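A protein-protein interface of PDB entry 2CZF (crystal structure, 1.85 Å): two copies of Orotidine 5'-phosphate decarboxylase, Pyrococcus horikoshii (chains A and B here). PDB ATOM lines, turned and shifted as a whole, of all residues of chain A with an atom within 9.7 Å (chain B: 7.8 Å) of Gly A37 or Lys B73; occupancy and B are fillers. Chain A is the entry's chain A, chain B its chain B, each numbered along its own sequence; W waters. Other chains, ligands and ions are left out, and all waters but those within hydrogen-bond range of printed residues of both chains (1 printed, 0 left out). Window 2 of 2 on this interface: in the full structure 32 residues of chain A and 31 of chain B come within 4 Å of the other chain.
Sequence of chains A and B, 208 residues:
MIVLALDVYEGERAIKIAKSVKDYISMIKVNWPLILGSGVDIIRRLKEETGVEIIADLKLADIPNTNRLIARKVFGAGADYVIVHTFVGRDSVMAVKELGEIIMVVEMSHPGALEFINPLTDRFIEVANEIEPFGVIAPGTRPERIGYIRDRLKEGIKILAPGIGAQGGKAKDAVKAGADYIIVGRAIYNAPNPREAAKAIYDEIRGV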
ATOM      1  N   VAL A   8     -11.028  -2.576 -19.470  1.00  0.00           N
ATOM      2  CA  VAL A   8     -12.113  -2.768 -18.526  1.00  0.00           C
ATOM      3  C   VAL A   8     -13.327  -2.255 -19.302  1.00  0.00           C
ATOM      4  O   VAL A   8     -13.813  -1.139 -19.078  1.00  0.00           O
ATOM      5  CB  VAL A   8     -11.919  -1.953 -17.217  1.00  0.00           C
ATOM      6  CG1 VAL A   8     -10.964  -2.686 -16.277  1.00  0.00           C
ATOM      7  CG2 VAL A   8     -11.373  -0.570 -17.536  1.00  0.00           C
ATOM      8  N   TYR A   9     -13.788  -3.099 -20.218  1.00  0.00           N
ATOM      9  CA  TYR A   9     -14.882  -2.830 -21.148  1.00  0.00           C
ATOM     10  C   TYR A   9     -16.245  -2.416 -20.620  1.00  0.00           C
ATOM     11  O   TYR A   9     -17.191  -2.251 -21.405  1.00  0.00           O
ATOM     12  CB  TYR A   9     -15.026  -4.040 -22.057  1.00  0.00           C
ATOM     13  CG  TYR A   9     -13.682  -4.568 -22.494  1.00  0.00           C
ATOM     14  CD1 TYR A   9     -12.816  -3.783 -23.250  1.00  0.00           C
ATOM     15  CD2 TYR A   9     -13.259  -5.842 -22.116  1.00  0.00           C
ATOM     16  CE1 TYR A   9     -11.560  -4.252 -23.621  1.00  0.00           C
ATOM     17  CE2 TYR A   9     -12.005  -6.320 -22.480  1.00  0.00           C
ATOM     18  CZ  TYR A   9     -11.162  -5.518 -23.231  1.00  0.00           C
ATOM     19  OH  TYR A   9      -9.918  -5.982 -23.588  1.00  0.00           O
ATOM     20  N   GLU A  10     -16.364  -2.254 -19.311  1.00  0.00           N
ATOM     21  CA  GLU A  10     -17.613  -1.818 -18.721  1.00  0.00           C
ATOM     22  C   GLU A  10     -17.495  -0.346 -18.430  1.00  0.00           C
ATOM     23  O   GLU A  10     -16.556   0.140 -17.762  1.00  0.00           O
ATOM     24  CB  GLU A  10     -17.961  -2.602 -17.457  1.00  0.00           C
ATOM     25  CG  GLU A  10     -17.558  -1.936 -16.152  1.00  0.00           C
ATOM     26  CD  GLU A  10     -18.651  -1.043 -15.558  1.00  0.00           C
ATOM     27  OE1 GLU A  10     -19.073  -0.064 -16.224  1.00  0.00           O
ATOM     28  OE2 GLU A  10     -19.084  -1.316 -14.418  1.00  0.00           O
ATOM     29  N   GLY A  11     -18.484   0.323 -18.988  1.00  0.00           N
ATOM     30  CA  GLY A  11     -18.681   1.746 -18.953  1.00  0.00           C
ATOM     31  C   GLY A  11     -18.040   2.538 -17.850  1.00  0.00           C
ATOM     32  O   GLY A  11     -16.844   2.424 -17.598  1.00  0.00           O
ATOM     33  N   GLU A  12     -18.832   3.335 -17.226  1.00  0.00           N
ATOM     34  CA  GLU A  12     -18.284   4.152 -16.168  1.00  0.00           C
ATOM     35  C   GLU A  12     -17.136   3.548 -15.292  1.00  0.00           C
ATOM     36  O   GLU A  12     -16.225   4.293 -14.960  1.00  0.00           O
ATOM     37  CB  GLU A  12     -19.445   4.698 -15.323  1.00  0.00           C
ATOM     38  CG  GLU A  12     -19.871   6.151 -15.632  1.00  0.00           C
ATOM     39  CD  GLU A  12     -20.583   6.338 -16.963  1.00  0.00           C
ATOM     40  OE1 GLU A  12     -21.175   7.428 -17.162  1.00  0.00           O
ATOM     41  OE2 GLU A  12     -20.550   5.418 -17.805  1.00  0.00           O
ATOM     42  N   ALA A  14     -14.640   1.797 -16.024  1.00  0.00           N
ATOM     43  CA  ALA A  14     -13.409   1.924 -16.795  1.00  0.00           C
ATOM     44  C   ALA A  14     -12.870   3.340 -16.624  1.00  0.00           C
ATOM     45  O   ALA A  14     -11.678   3.536 -16.393  1.00  0.00           O
ATOM     46  CB  ALA A  14     -13.682   1.644 -18.265  1.00  0.00           C
ATOM     47  N   ASN A  31      -9.020  -0.034 -26.952  1.00  0.00           N
ATOM     48  CA  ASN A  31      -9.104  -0.970 -28.063  1.00  0.00           C
ATOM     49  C   ASN A  31     -10.500  -1.024 -28.691  1.00  0.00           C
ATOM     50  O   ASN A  31     -11.414  -0.285 -28.288  1.00  0.00           O
ATOM     51  CB  ASN A  31      -8.695  -2.365 -27.585  1.00  0.00           C
ATOM     52  CG  ASN A  31      -9.511  -2.828 -26.397  1.00  0.00           C
ATOM     53  OD1 ASN A  31     -10.619  -2.326 -26.148  1.00  0.00           O
ATOM     54  ND2 ASN A  31      -8.980  -3.801 -25.660  1.00  0.00           N
ATOM     55  N   TRP A  32     -10.669  -1.896 -29.686  1.00  0.00           N
ATOM     56  CA  TRP A  32     -11.967  -2.004 -30.334  1.00  0.00           C
ATOM     57  C   TRP A  32     -13.098  -2.417 -29.389  1.00  0.00           C
ATOM     58  O   TRP A  32     -14.191  -1.860 -29.464  1.00  0.00           O
ATOM     59  CB  TRP A  32     -11.919  -2.979 -31.509  1.00  0.00           C
ATOM     60  CG  TRP A  32     -11.296  -2.418 -32.757  1.00  0.00           C
ATOM     61  CD1 TRP A  32     -10.241  -2.944 -33.445  1.00  0.00           C
ATOM     62  CD2 TRP A  32     -11.735  -1.267 -33.509  1.00  0.00           C
ATOM     63  NE1 TRP A  32      -9.997  -2.201 -34.580  1.00  0.00           N
ATOM     64  CE2 TRP A  32     -10.895  -1.167 -34.646  1.00  0.00           C
ATOM     65  CE3 TRP A  32     -12.754  -0.317 -33.336  1.00  0.00           C
ATOM     66  CZ2 TRP A  32     -11.044  -0.145 -35.615  1.00  0.00           C
ATOM     67  CZ3 TRP A  32     -12.905   0.701 -34.301  1.00  0.00           C
ATOM     68  CH2 TRP A  32     -12.048   0.771 -35.424  1.00  0.00           C
ATOM     69  N   PRO A  33     -12.863  -3.391 -28.486  1.00  0.00           N
ATOM     70  CA  PRO A  33     -13.971  -3.772 -27.597  1.00  0.00           C
ATOM     71  C   PRO A  33     -14.576  -2.602 -26.824  1.00  0.00           C
ATOM     72  O   PRO A  33     -15.794  -2.447 -26.791  1.00  0.00           O
ATOM     73  CB  PRO A  33     -13.338  -4.834 -26.693  1.00  0.00           C
ATOM     74  CG  PRO A  33     -12.344  -5.495 -27.635  1.00  0.00           C
ATOM     75  CD  PRO A  33     -11.702  -4.275 -28.280  1.00  0.00           C
ATOM     76  N   LEU A  34     -13.729  -1.772 -26.220  1.00  0.00           N
ATOM     77  CA  LEU A  34     -14.213  -0.619 -25.458  1.00  0.00           C
ATOM     78  C   LEU A  34     -14.997   0.311 -26.367  1.00  0.00           C
ATOM     79  O   LEU A  34     -16.086   0.774 -26.017  1.00  0.00           O
ATOM     80  CB  LEU A  34     -13.043   0.155 -24.834  1.00  0.00           C
ATOM     81  CG  LEU A  34     -13.425   1.444 -24.097  1.00  0.00           C
ATOM     82  CD1 LEU A  34     -14.566   1.175 -23.130  1.00  0.00           C
ATOM     83  CD2 LEU A  34     -12.209   1.987 -23.358  1.00  0.00           C
ATOM     84  N   ILE A  35     -14.435   0.576 -27.543  1.00  0.00           N
ATOM     85  CA  ILE A  35     -15.056   1.443 -28.534  1.00  0.00           C
ATOM     86  C   ILE A  35     -16.423   0.902 -28.975  1.00  0.00           C
ATOM     87  O   ILE A  35     -17.388   1.660 -29.124  1.00  0.00           O
ATOM     88  CB  ILE A  35     -14.131   1.600 -29.762  1.00  0.00           C
ATOM     89  CG1 ILE A  35     -12.935   2.473 -29.384  1.00  0.00           C
ATOM     90  CG2 ILE A  35     -14.891   2.184 -30.940  1.00  0.00           C
ATOM     91  CD1 ILE A  35     -11.918   2.666 -30.494  1.00  0.00           C
ATOM     92  N   LEU A  36     -16.499  -0.408 -29.179  1.00  0.00           N
ATOM     93  CA  LEU A  36     -17.741  -1.038 -29.587  1.00  0.00           C
ATOM     94  C   LEU A  36     -18.759  -0.972 -28.459  1.00  0.00           C
ATOM     95  O   LEU A  36     -19.925  -0.636 -28.683  1.00  0.00           O
ATOM     96  CB  LEU A  36     -17.488  -2.498 -29.961  1.00  0.00           C
ATOM     97  CG  LEU A  36     -16.856  -2.724 -31.332  1.00  0.00           C
ATOM     98  CD1 LEU A  36     -16.191  -4.102 -31.381  1.00  0.00           C
ATOM     99  CD2 LEU A  36     -17.937  -2.589 -32.398  1.00  0.00           C
ATOM    100  N   GLY A  37     -18.306  -1.288 -27.248  1.00  0.00           N
ATOM    101  CA  GLY A  37     -19.186  -1.285 -26.091  1.00  0.00           C
ATOM    102  C   GLY A  37     -19.658   0.074 -25.606  1.00  0.00           C
ATOM    103  O   GLY A  37     -20.783   0.202 -25.123  1.00  0.00           O
ATOM    104  N   SER A  38     -18.823   1.097 -25.732  1.00  0.00           N
ATOM    105  CA  SER A  38     -19.199   2.430 -25.264  1.00  0.00           C
ATOM    106  C   SER A  38     -19.390   3.459 -26.369  1.00  0.00           C
ATOM    107  O   SER A  38     -19.931   4.535 -26.133  1.00  0.00           O
ATOM    108  CB  SER A  38     -18.146   2.954 -24.283  1.00  0.00           C
ATOM    109  OG  SER A  38     -18.057   2.132 -23.141  1.00  0.00           O
ATOM    110  N   GLY A  39     -18.949   3.137 -27.576  1.00  0.00           N
ATOM    111  CA  GLY A  39     -19.067   4.087 -28.665  1.00  0.00           C
ATOM    112  C   GLY A  39     -17.758   4.843 -28.767  1.00  0.00           C
ATOM    113  O   GLY A  39     -17.031   4.957 -27.784  1.00  0.00           O
ATOM    114  N   VAL A  40     -17.447   5.358 -29.948  1.00  0.00           N
ATOM    115  CA  VAL A  40     -16.201   6.087 -30.134  1.00  0.00           C
ATOM    116  C   VAL A  40     -16.130   7.304 -29.205  1.00  0.00           C
ATOM    117  O   VAL A  40     -15.091   7.957 -29.094  1.00  0.00           O
ATOM    118  CB  VAL A  40     -16.036   6.524 -31.617  1.00  0.00           C
ATOM    119  CG1 VAL A  40     -17.075   7.561 -31.985  1.00  0.00           C
ATOM    120  CG2 VAL A  40     -14.632   7.051 -31.857  1.00  0.00           C
ATOM    121  N   ASP A  41     -17.232   7.594 -28.524  1.00  0.00           N
ATOM    122  CA  ASP A  41     -17.283   8.731 -27.610  1.00  0.00           C
ATOM    123  C   ASP A  41     -16.462   8.503 -26.354  1.00  0.00           C
ATOM    124  O   ASP A  41     -15.954   9.454 -25.760  1.00  0.00           O
ATOM    125  CB  ASP A  41     -18.728   9.029 -27.209  1.00  0.00           C
ATOM    126  CG  ASP A  41     -19.572   9.468 -28.380  1.00  0.00           C
ATOM    127  OD1 ASP A  41     -19.170  10.430 -29.069  1.00  0.00           O
ATOM    128  OD2 ASP A  41     -20.635   8.851 -28.608  1.00  0.00           O
ATOM    129  N   ILE A  42     -16.341   7.247 -25.937  1.00  0.00           N
ATOM    130  CA  ILE A  42     -15.572   6.934 -24.743  1.00  0.00           C
ATOM    131  C   ILE A  42     -14.181   7.554 -24.887  1.00  0.00           C
ATOM    132  O   ILE A  42     -13.463   7.706 -23.904  1.00  0.00           O
ATOM    133  CB  ILE A  42     -15.456   5.399 -24.530  1.00  0.00           C
ATOM    134  CG1 ILE A  42     -14.872   5.099 -23.149  1.00  0.00           C
ATOM    135  CG2 ILE A  42     -14.576   4.780 -25.599  1.00  0.00           C
ATOM    136  CD1 ILE A  42     -15.751   5.555 -22.002  1.00  0.00           C
ATOM    137  N   VAL B  40     -22.518  -0.151 -33.335  1.00  0.00           N
ATOM    138  CA  VAL B  40     -22.571  -1.531 -33.841  1.00  0.00           C
ATOM    139  C   VAL B  40     -23.984  -2.094 -33.951  1.00  0.00           C
ATOM    140  O   VAL B  40     -24.200  -3.118 -34.596  1.00  0.00           O
ATOM    141  CB  VAL B  40     -21.719  -2.505 -32.963  1.00  0.00           C
ATOM    142  CG1 VAL B  40     -22.380  -2.729 -31.610  1.00  0.00           C
ATOM    143  CG2 VAL B  40     -21.538  -3.837 -33.684  1.00  0.00           C
ATOM    144  N   ASP B  41     -24.940  -1.434 -33.305  1.00  0.00           N
ATOM    145  CA  ASP B  41     -26.334  -1.879 -33.348  1.00  0.00           C
ATOM    146  C   ASP B  41     -26.924  -1.674 -34.747  1.00  0.00           C
ATOM    147  O   ASP B  41     -27.996  -2.205 -35.070  1.00  0.00           O
ATOM    148  CB  ASP B  41     -27.162  -1.111 -32.304  1.00  0.00           C
ATOM    149  CG  ASP B  41     -28.648  -1.432 -32.377  1.00  0.00           C
ATOM    150  OD1 ASP B  41     -29.450  -0.483 -32.518  1.00  0.00           O
ATOM    151  OD2 ASP B  41     -29.018  -2.625 -32.293  1.00  0.00           O
ATOM    152  N   ILE B  43     -26.023  -2.996 -37.264  1.00  0.00           N
ATOM    153  CA  ILE B  43     -26.035  -4.299 -37.911  1.00  0.00           C
ATOM    154  C   ILE B  43     -27.403  -4.935 -37.677  1.00  0.00           C
ATOM    155  O   ILE B  43     -28.005  -5.476 -38.598  1.00  0.00           O
ATOM    156  CB  ILE B  43     -24.921  -5.217 -37.348  1.00  0.00           C
ATOM    157  CG1 ILE B  43     -23.551  -4.676 -37.772  1.00  0.00           C
ATOM    158  CG2 ILE B  43     -25.105  -6.655 -37.846  1.00  0.00           C
ATOM    159  CD1 ILE B  43     -22.376  -5.457 -37.212  1.00  0.00           C
ATOM    160  N   LEU B  58     -14.336  -6.308 -40.959  1.00  0.00           N
ATOM    161  CA  LEU B  58     -13.472  -5.689 -39.961  1.00  0.00           C
ATOM    162  C   LEU B  58     -11.978  -5.903 -40.207  1.00  0.00           C
ATOM    163  O   LEU B  58     -11.158  -5.120 -39.739  1.00  0.00           O
ATOM    164  CB  LEU B  58     -13.834  -6.233 -38.570  1.00  0.00           C
ATOM    165  CG  LEU B  58     -15.326  -6.263 -38.207  1.00  0.00           C
ATOM    166  CD1 LEU B  58     -15.513  -6.791 -36.807  1.00  0.00           C
ATOM    167  CD2 LEU B  58     -15.906  -4.882 -38.331  1.00  0.00           C
ATOM    168  N   ASN B  67      -9.188 -10.731 -30.703  1.00  0.00           N
ATOM    169  CA  ASN B  67      -9.983 -11.032 -31.876  1.00  0.00           C
ATOM    170  C   ASN B  67     -11.299 -11.670 -31.382  1.00  0.00           C
ATOM    171  O   ASN B  67     -12.375 -11.410 -31.919  1.00  0.00           O
ATOM    172  CB  ASN B  67      -9.242 -12.036 -32.766  1.00  0.00           C
ATOM    173  CG  ASN B  67      -8.475 -11.378 -33.900  1.00  0.00           C
ATOM    174  OD1 ASN B  67      -8.189 -10.177 -33.873  1.00  0.00           O
ATOM    175  ND2 ASN B  67      -8.127 -12.180 -34.907  1.00  0.00           N
ATOM    176  N   ARG B  68     -11.213 -12.509 -30.354  1.00  0.00           N
ATOM    177  CA  ARG B  68     -12.420 -13.181 -29.854  1.00  0.00           C
ATOM    178  C   ARG B  68     -13.393 -12.187 -29.217  1.00  0.00           C
ATOM    179  O   ARG B  68     -14.599 -12.264 -29.429  1.00  0.00           O
ATOM    180  CB  ARG B  68     -12.044 -14.279 -28.849  1.00  0.00           C
ATOM    181  CG  ARG B  68     -13.139 -15.326 -28.631  1.00  0.00           C
ATOM    182  CD  ARG B  68     -12.722 -16.378 -27.601  1.00  0.00           C
ATOM    183  NE  ARG B  68     -11.525 -17.124 -27.998  1.00  0.00           N
ATOM    184  CZ  ARG B  68     -10.318 -16.958 -27.461  1.00  0.00           C
ATOM    185  NH1 ARG B  68     -10.129 -16.073 -26.490  1.00  0.00           N
ATOM    186  NH2 ARG B  68      -9.295 -17.674 -27.898  1.00  0.00           N
ATOM    187  N   LEU B  69     -12.865 -11.263 -28.422  1.00  0.00           N
ATOM    188  CA  LEU B  69     -13.691 -10.245 -27.782  1.00  0.00           C
ATOM    189  C   LEU B  69     -14.432  -9.443 -28.845  1.00  0.00           C
ATOM    190  O   LEU B  69     -15.639  -9.219 -28.750  1.00  0.00           O
ATOM    191  CB  LEU B  69     -12.814  -9.304 -26.949  1.00  0.00           C
ATOM    192  CG  LEU B  69     -12.417  -9.797 -25.552  1.00  0.00           C
ATOM    193  CD1 LEU B  69     -11.078  -9.178 -25.132  1.00  0.00           C
ATOM    194  CD2 LEU B  69     -13.536  -9.443 -24.558  1.00  0.00           C
ATOM    195  N   ILE B  70     -13.711  -9.023 -29.878  1.00  0.00           N
ATOM    196  CA  ILE B  70     -14.341  -8.236 -30.931  1.00  0.00           C
ATOM    197  C   ILE B  70     -15.407  -9.066 -31.653  1.00  0.00           C
ATOM    198  O   ILE B  70     -16.539  -8.619 -31.843  1.00  0.00           O
ATOM    199  CB  ILE B  70     -13.282  -7.720 -31.942  1.00  0.00           C
ATOM    200  CG1 ILE B  70     -12.263  -6.826 -31.213  1.00  0.00           C
ATOM    201  CG2 ILE B  70     -13.967  -6.902 -33.039  1.00  0.00           C
ATOM    202  CD1 ILE B  70     -11.056  -6.422 -32.069  1.00  0.00           C
ATOM    203  N   ALA B  71     -15.045 -10.283 -32.037  1.00  0.00           N
ATOM    204  CA  ALA B  71     -15.978 -11.154 -32.741  1.00  0.00           C
ATOM    205  C   ALA B  71     -17.216 -11.436 -31.903  1.00  0.00           C
ATOM    206  O   ALA B  71     -18.332 -11.397 -32.413  1.00  0.00           O
ATOM    207  CB  ALA B  71     -15.292 -12.461 -33.118  1.00  0.00           C
ATOM    208  N   ARG B  72     -17.027 -11.722 -30.618  1.00  0.00           N
ATOM    209  CA  ARG B  72     -18.170 -11.994 -29.756  1.00  0.00           C
ATOM    210  C   ARG B  72     -19.141 -10.824 -29.823  1.00  0.00           C
ATOM    211  O   ARG B  72     -20.346 -11.009 -30.006  1.00  0.00           O
ATOM    212  CB  ARG B  72     -17.719 -12.218 -28.302  1.00  0.00           C
ATOM    213  CG  ARG B  72     -18.846 -12.669 -27.393  1.00  0.00           C
ATOM    214  CD  ARG B  72     -18.346 -12.987 -25.991  1.00  0.00           C
ATOM    215  NE  ARG B  72     -17.422 -14.118 -25.983  1.00  0.00           N
ATOM    216  CZ  ARG B  72     -16.179 -14.075 -25.511  1.00  0.00           C
ATOM    217  NH1 ARG B  72     -15.687 -12.950 -24.996  1.00  0.00           N
ATOM    218  NH2 ARG B  72     -15.429 -15.163 -25.550  1.00  0.00           N
ATOM    219  N   LYS B  73     -18.621  -9.613 -29.687  1.00  0.00           N
ATOM    220  CA  LYS B  73     -19.488  -8.447 -29.745  1.00  0.00           C
ATOM    221  C   LYS B  73     -20.167  -8.249 -31.091  1.00  0.00           C
ATOM    222  O   LYS B  73     -21.367  -7.957 -31.153  1.00  0.00           O
ATOM    223  CB  LYS B  73     -18.712  -7.175 -29.403  1.00  0.00           C
ATOM    224  CG  LYS B  73     -18.597  -6.922 -27.918  1.00  0.00           C
ATOM    225  CD  LYS B  73     -18.439  -5.435 -27.629  1.00  0.00           C
ATOM    226  CE  LYS B  73     -19.581  -4.621 -28.252  1.00  0.00           C
ATOM    227  NZ  LYS B  73     -20.934  -5.040 -27.777  1.00  0.00           N
ATOM    228  N   VAL B  74     -19.407  -8.408 -32.173  1.00  0.00           N
ATOM    229  CA  VAL B  74     -19.955  -8.197 -33.501  1.00  0.00           C
ATOM    230  C   VAL B  74     -20.916  -9.298 -33.941  1.00  0.00           C
ATOM    231  O   VAL B  74     -21.970  -8.995 -34.490  1.00  0.00           O
ATOM    232  CB  VAL B  74     -18.813  -7.979 -34.524  1.00  0.00           C
ATOM    233  CG1 VAL B  74     -19.371  -7.777 -35.927  1.00  0.00           C
ATOM    234  CG2 VAL B  74     -18.008  -6.745 -34.109  1.00  0.00           C
ATOM    235  N   PHE B  75     -20.586 -10.566 -33.704  1.00  0.00           N
ATOM    236  CA  PHE B  75     -21.524 -11.632 -34.062  1.00  0.00           C
ATOM    237  C   PHE B  75     -22.756 -11.439 -33.159  1.00  0.00           C
ATOM    238  O   PHE B  75     -23.902 -11.631 -33.581  1.00  0.00           O
ATOM    239  CB  PHE B  75     -20.931 -13.012 -33.776  1.00  0.00           C
ATOM    240  CG  PHE B  75     -19.980 -13.508 -34.831  1.00  0.00           C
ATOM    241  CD1 PHE B  75     -20.395 -13.645 -36.153  1.00  0.00           C
ATOM    242  CD2 PHE B  75     -18.669 -13.862 -34.499  1.00  0.00           C
ATOM    243  CE1 PHE B  75     -19.522 -14.126 -37.136  1.00  0.00           C
ATOM    244  CE2 PHE B  75     -17.788 -14.344 -35.473  1.00  0.00           C
ATOM    245  CZ  PHE B  75     -18.224 -14.474 -36.797  1.00  0.00           C
ATOM    246  N   GLY B  76     -22.499 -11.056 -31.911  1.00  0.00           N
ATOM    247  CA  GLY B  76     -23.578 -10.849 -30.964  1.00  0.00           C
ATOM    248  C   GLY B  76     -24.504  -9.731 -31.388  1.00  0.00           C
ATOM    249  O   GLY B  76     -25.695  -9.759 -31.089  1.00  0.00           O
ATOM    250  N   ALA B  77     -23.948  -8.742 -32.083  1.00  0.00           N
ATOM    251  CA  ALA B  77     -24.719  -7.600 -32.577  1.00  0.00           C
ATOM    252  C   ALA B  77     -25.519  -7.993 -33.819  1.00  0.00           C
ATOM    253  O   ALA B  77     -26.264  -7.184 -34.369  1.00  0.00           O
ATOM    254  CB  ALA B  77     -23.780  -6.438 -32.907  1.00  0.00           C
ATOM    255  N   GLY B  78     -25.355  -9.229 -34.278  1.00  0.00           N
ATOM    256  CA  GLY B  78     -26.115  -9.642 -35.442  1.00  0.00           C
ATOM    257  C   GLY B  78     -25.341  -9.921 -36.716  1.00  0.00           C
ATOM    258  O   GLY B  78     -25.949 -10.246 -37.734  1.00  0.00           O
ATOM    259  N   ALA B  79     -24.018  -9.811 -36.684  1.00  0.00           N
ATOM    260  CA  ALA B  79     -23.235 -10.087 -37.891  1.00  0.00           C
ATOM    261  C   ALA B  79     -23.327 -11.579 -38.205  1.00  0.00           C
ATOM    262  O   ALA B  79     -23.365 -12.414 -37.303  1.00  0.00           O
ATOM    263  CB  ALA B  79     -21.765  -9.693 -37.684  1.00  0.00           C
ATOM    264  N   VAL B  82     -17.682 -12.472 -40.429  1.00  0.00           N
ATOM    265  CA  VAL B  82     -16.680 -11.482 -40.079  1.00  0.00           C
ATOM    266  C   VAL B  82     -15.475 -11.725 -40.988  1.00  0.00           C
ATOM    267  O   VAL B  82     -15.054 -12.865 -41.179  1.00  0.00           O
ATOM    268  CB  VAL B  82     -16.235 -11.609 -38.615  1.00  0.00           C
ATOM    269  CG1 VAL B  82     -15.018 -10.732 -38.383  1.00  0.00           C
ATOM    270  CG2 VAL B  82     -17.372 -11.174 -37.675  1.00  0.00           C
ATOM    271  N   LEU B  99     -16.525 -18.630 -33.019  1.00  0.00           N
ATOM    272  CA  LEU B  99     -17.722 -17.886 -32.620  1.00  0.00           C
ATOM    273  C   LEU B  99     -18.714 -17.623 -33.751  1.00  0.00           C
ATOM    274  O   LEU B  99     -19.871 -17.270 -33.506  1.00  0.00           O
ATOM    275  CB  LEU B  99     -17.324 -16.552 -31.983  1.00  0.00           C
ATOM    276  CG  LEU B  99     -16.346 -16.660 -30.810  1.00  0.00           C
ATOM    277  CD1 LEU B  99     -16.249 -15.324 -30.100  1.00  0.00           C
ATOM    278  CD2 LEU B  99     -16.827 -17.739 -29.845  1.00  0.00           C
HETATM  279  O   HOH W   1     -21.008   0.581 -31.041  1.00  0.00           O
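The side-chain hydroxyl (OH) of Tyr A9 sits at hydrogen-bond distance from the side-chain amide nitrogen (ND2) of Asn A31 (3.2 Å).
OH of Tyr A9 touches CD1 of Leu B69, at 3.7 Å.
Trp A32 touches Ile B70.
Leu B69 touches Pro A33 (CB to CG, 3.9 Å).
CG1 of Ile B70 touches CG of Pro A33 (3.8 Å).
CD2 of Leu A36 touches CB of Val B40, at 3.8 Å.
Leu A36 touches Ile B70 (CD1 to CG2, 3.9 Å).
CB of Leu A36 touches CE of Lys B73 (3.4 Å).
Gly A37 touches Lys B73 (N to CE, 3.7 Å).
Of the printed residues of chain B, Tyr A9 touches Leu B69 (3.7 Å).
Leu A34 touches none of the printed residues of chain B.
Of chain B, only Lys B73 (3.7 Å) comes within 4 Å of Gly A37.
Val A40 touches none of the printed residues of chain B.
Printed residues of chain A within 4 Å of Leu B69: Tyr A9 and Pro A33.
No residue of chain A comes within 4 Å of Ala B71.
Of chain A, only Leu A36 and Gly A37 come within 4 Å of Lys B73.
No residue of chain A comes within 4 Å of Gly B76.
The nearest residue of chain A that does not touch Lys B73 is Pro A33 (4.1 Å).
Of the 18 printed residues of chain A, 5 touch a printed residue of chain B.
Hydrophobic or aromatic side chains of chain A that line the printed part of chain B: Tyr A9, Trp A32, Pro A33 and Leu A36.
Hydrophobic or aromatic side chains of chain B within 4 Å of the printed part of chain A: Val B40, Leu B69 and Ile B70.
Among the printed residues, 8 pairs touch across the chains.
Among the printed residues, no Asp or Glu carboxylate lies within 4 Å of a Lys or Arg side-chain nitrogen of the other chain.
Positions printed for both chains: 40 and 41.
Water W1 bridges the backbone NH of Val B40 (2.8 Å) and the backbone carbonyl oxygen of Leu A36 (2.9 Å).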
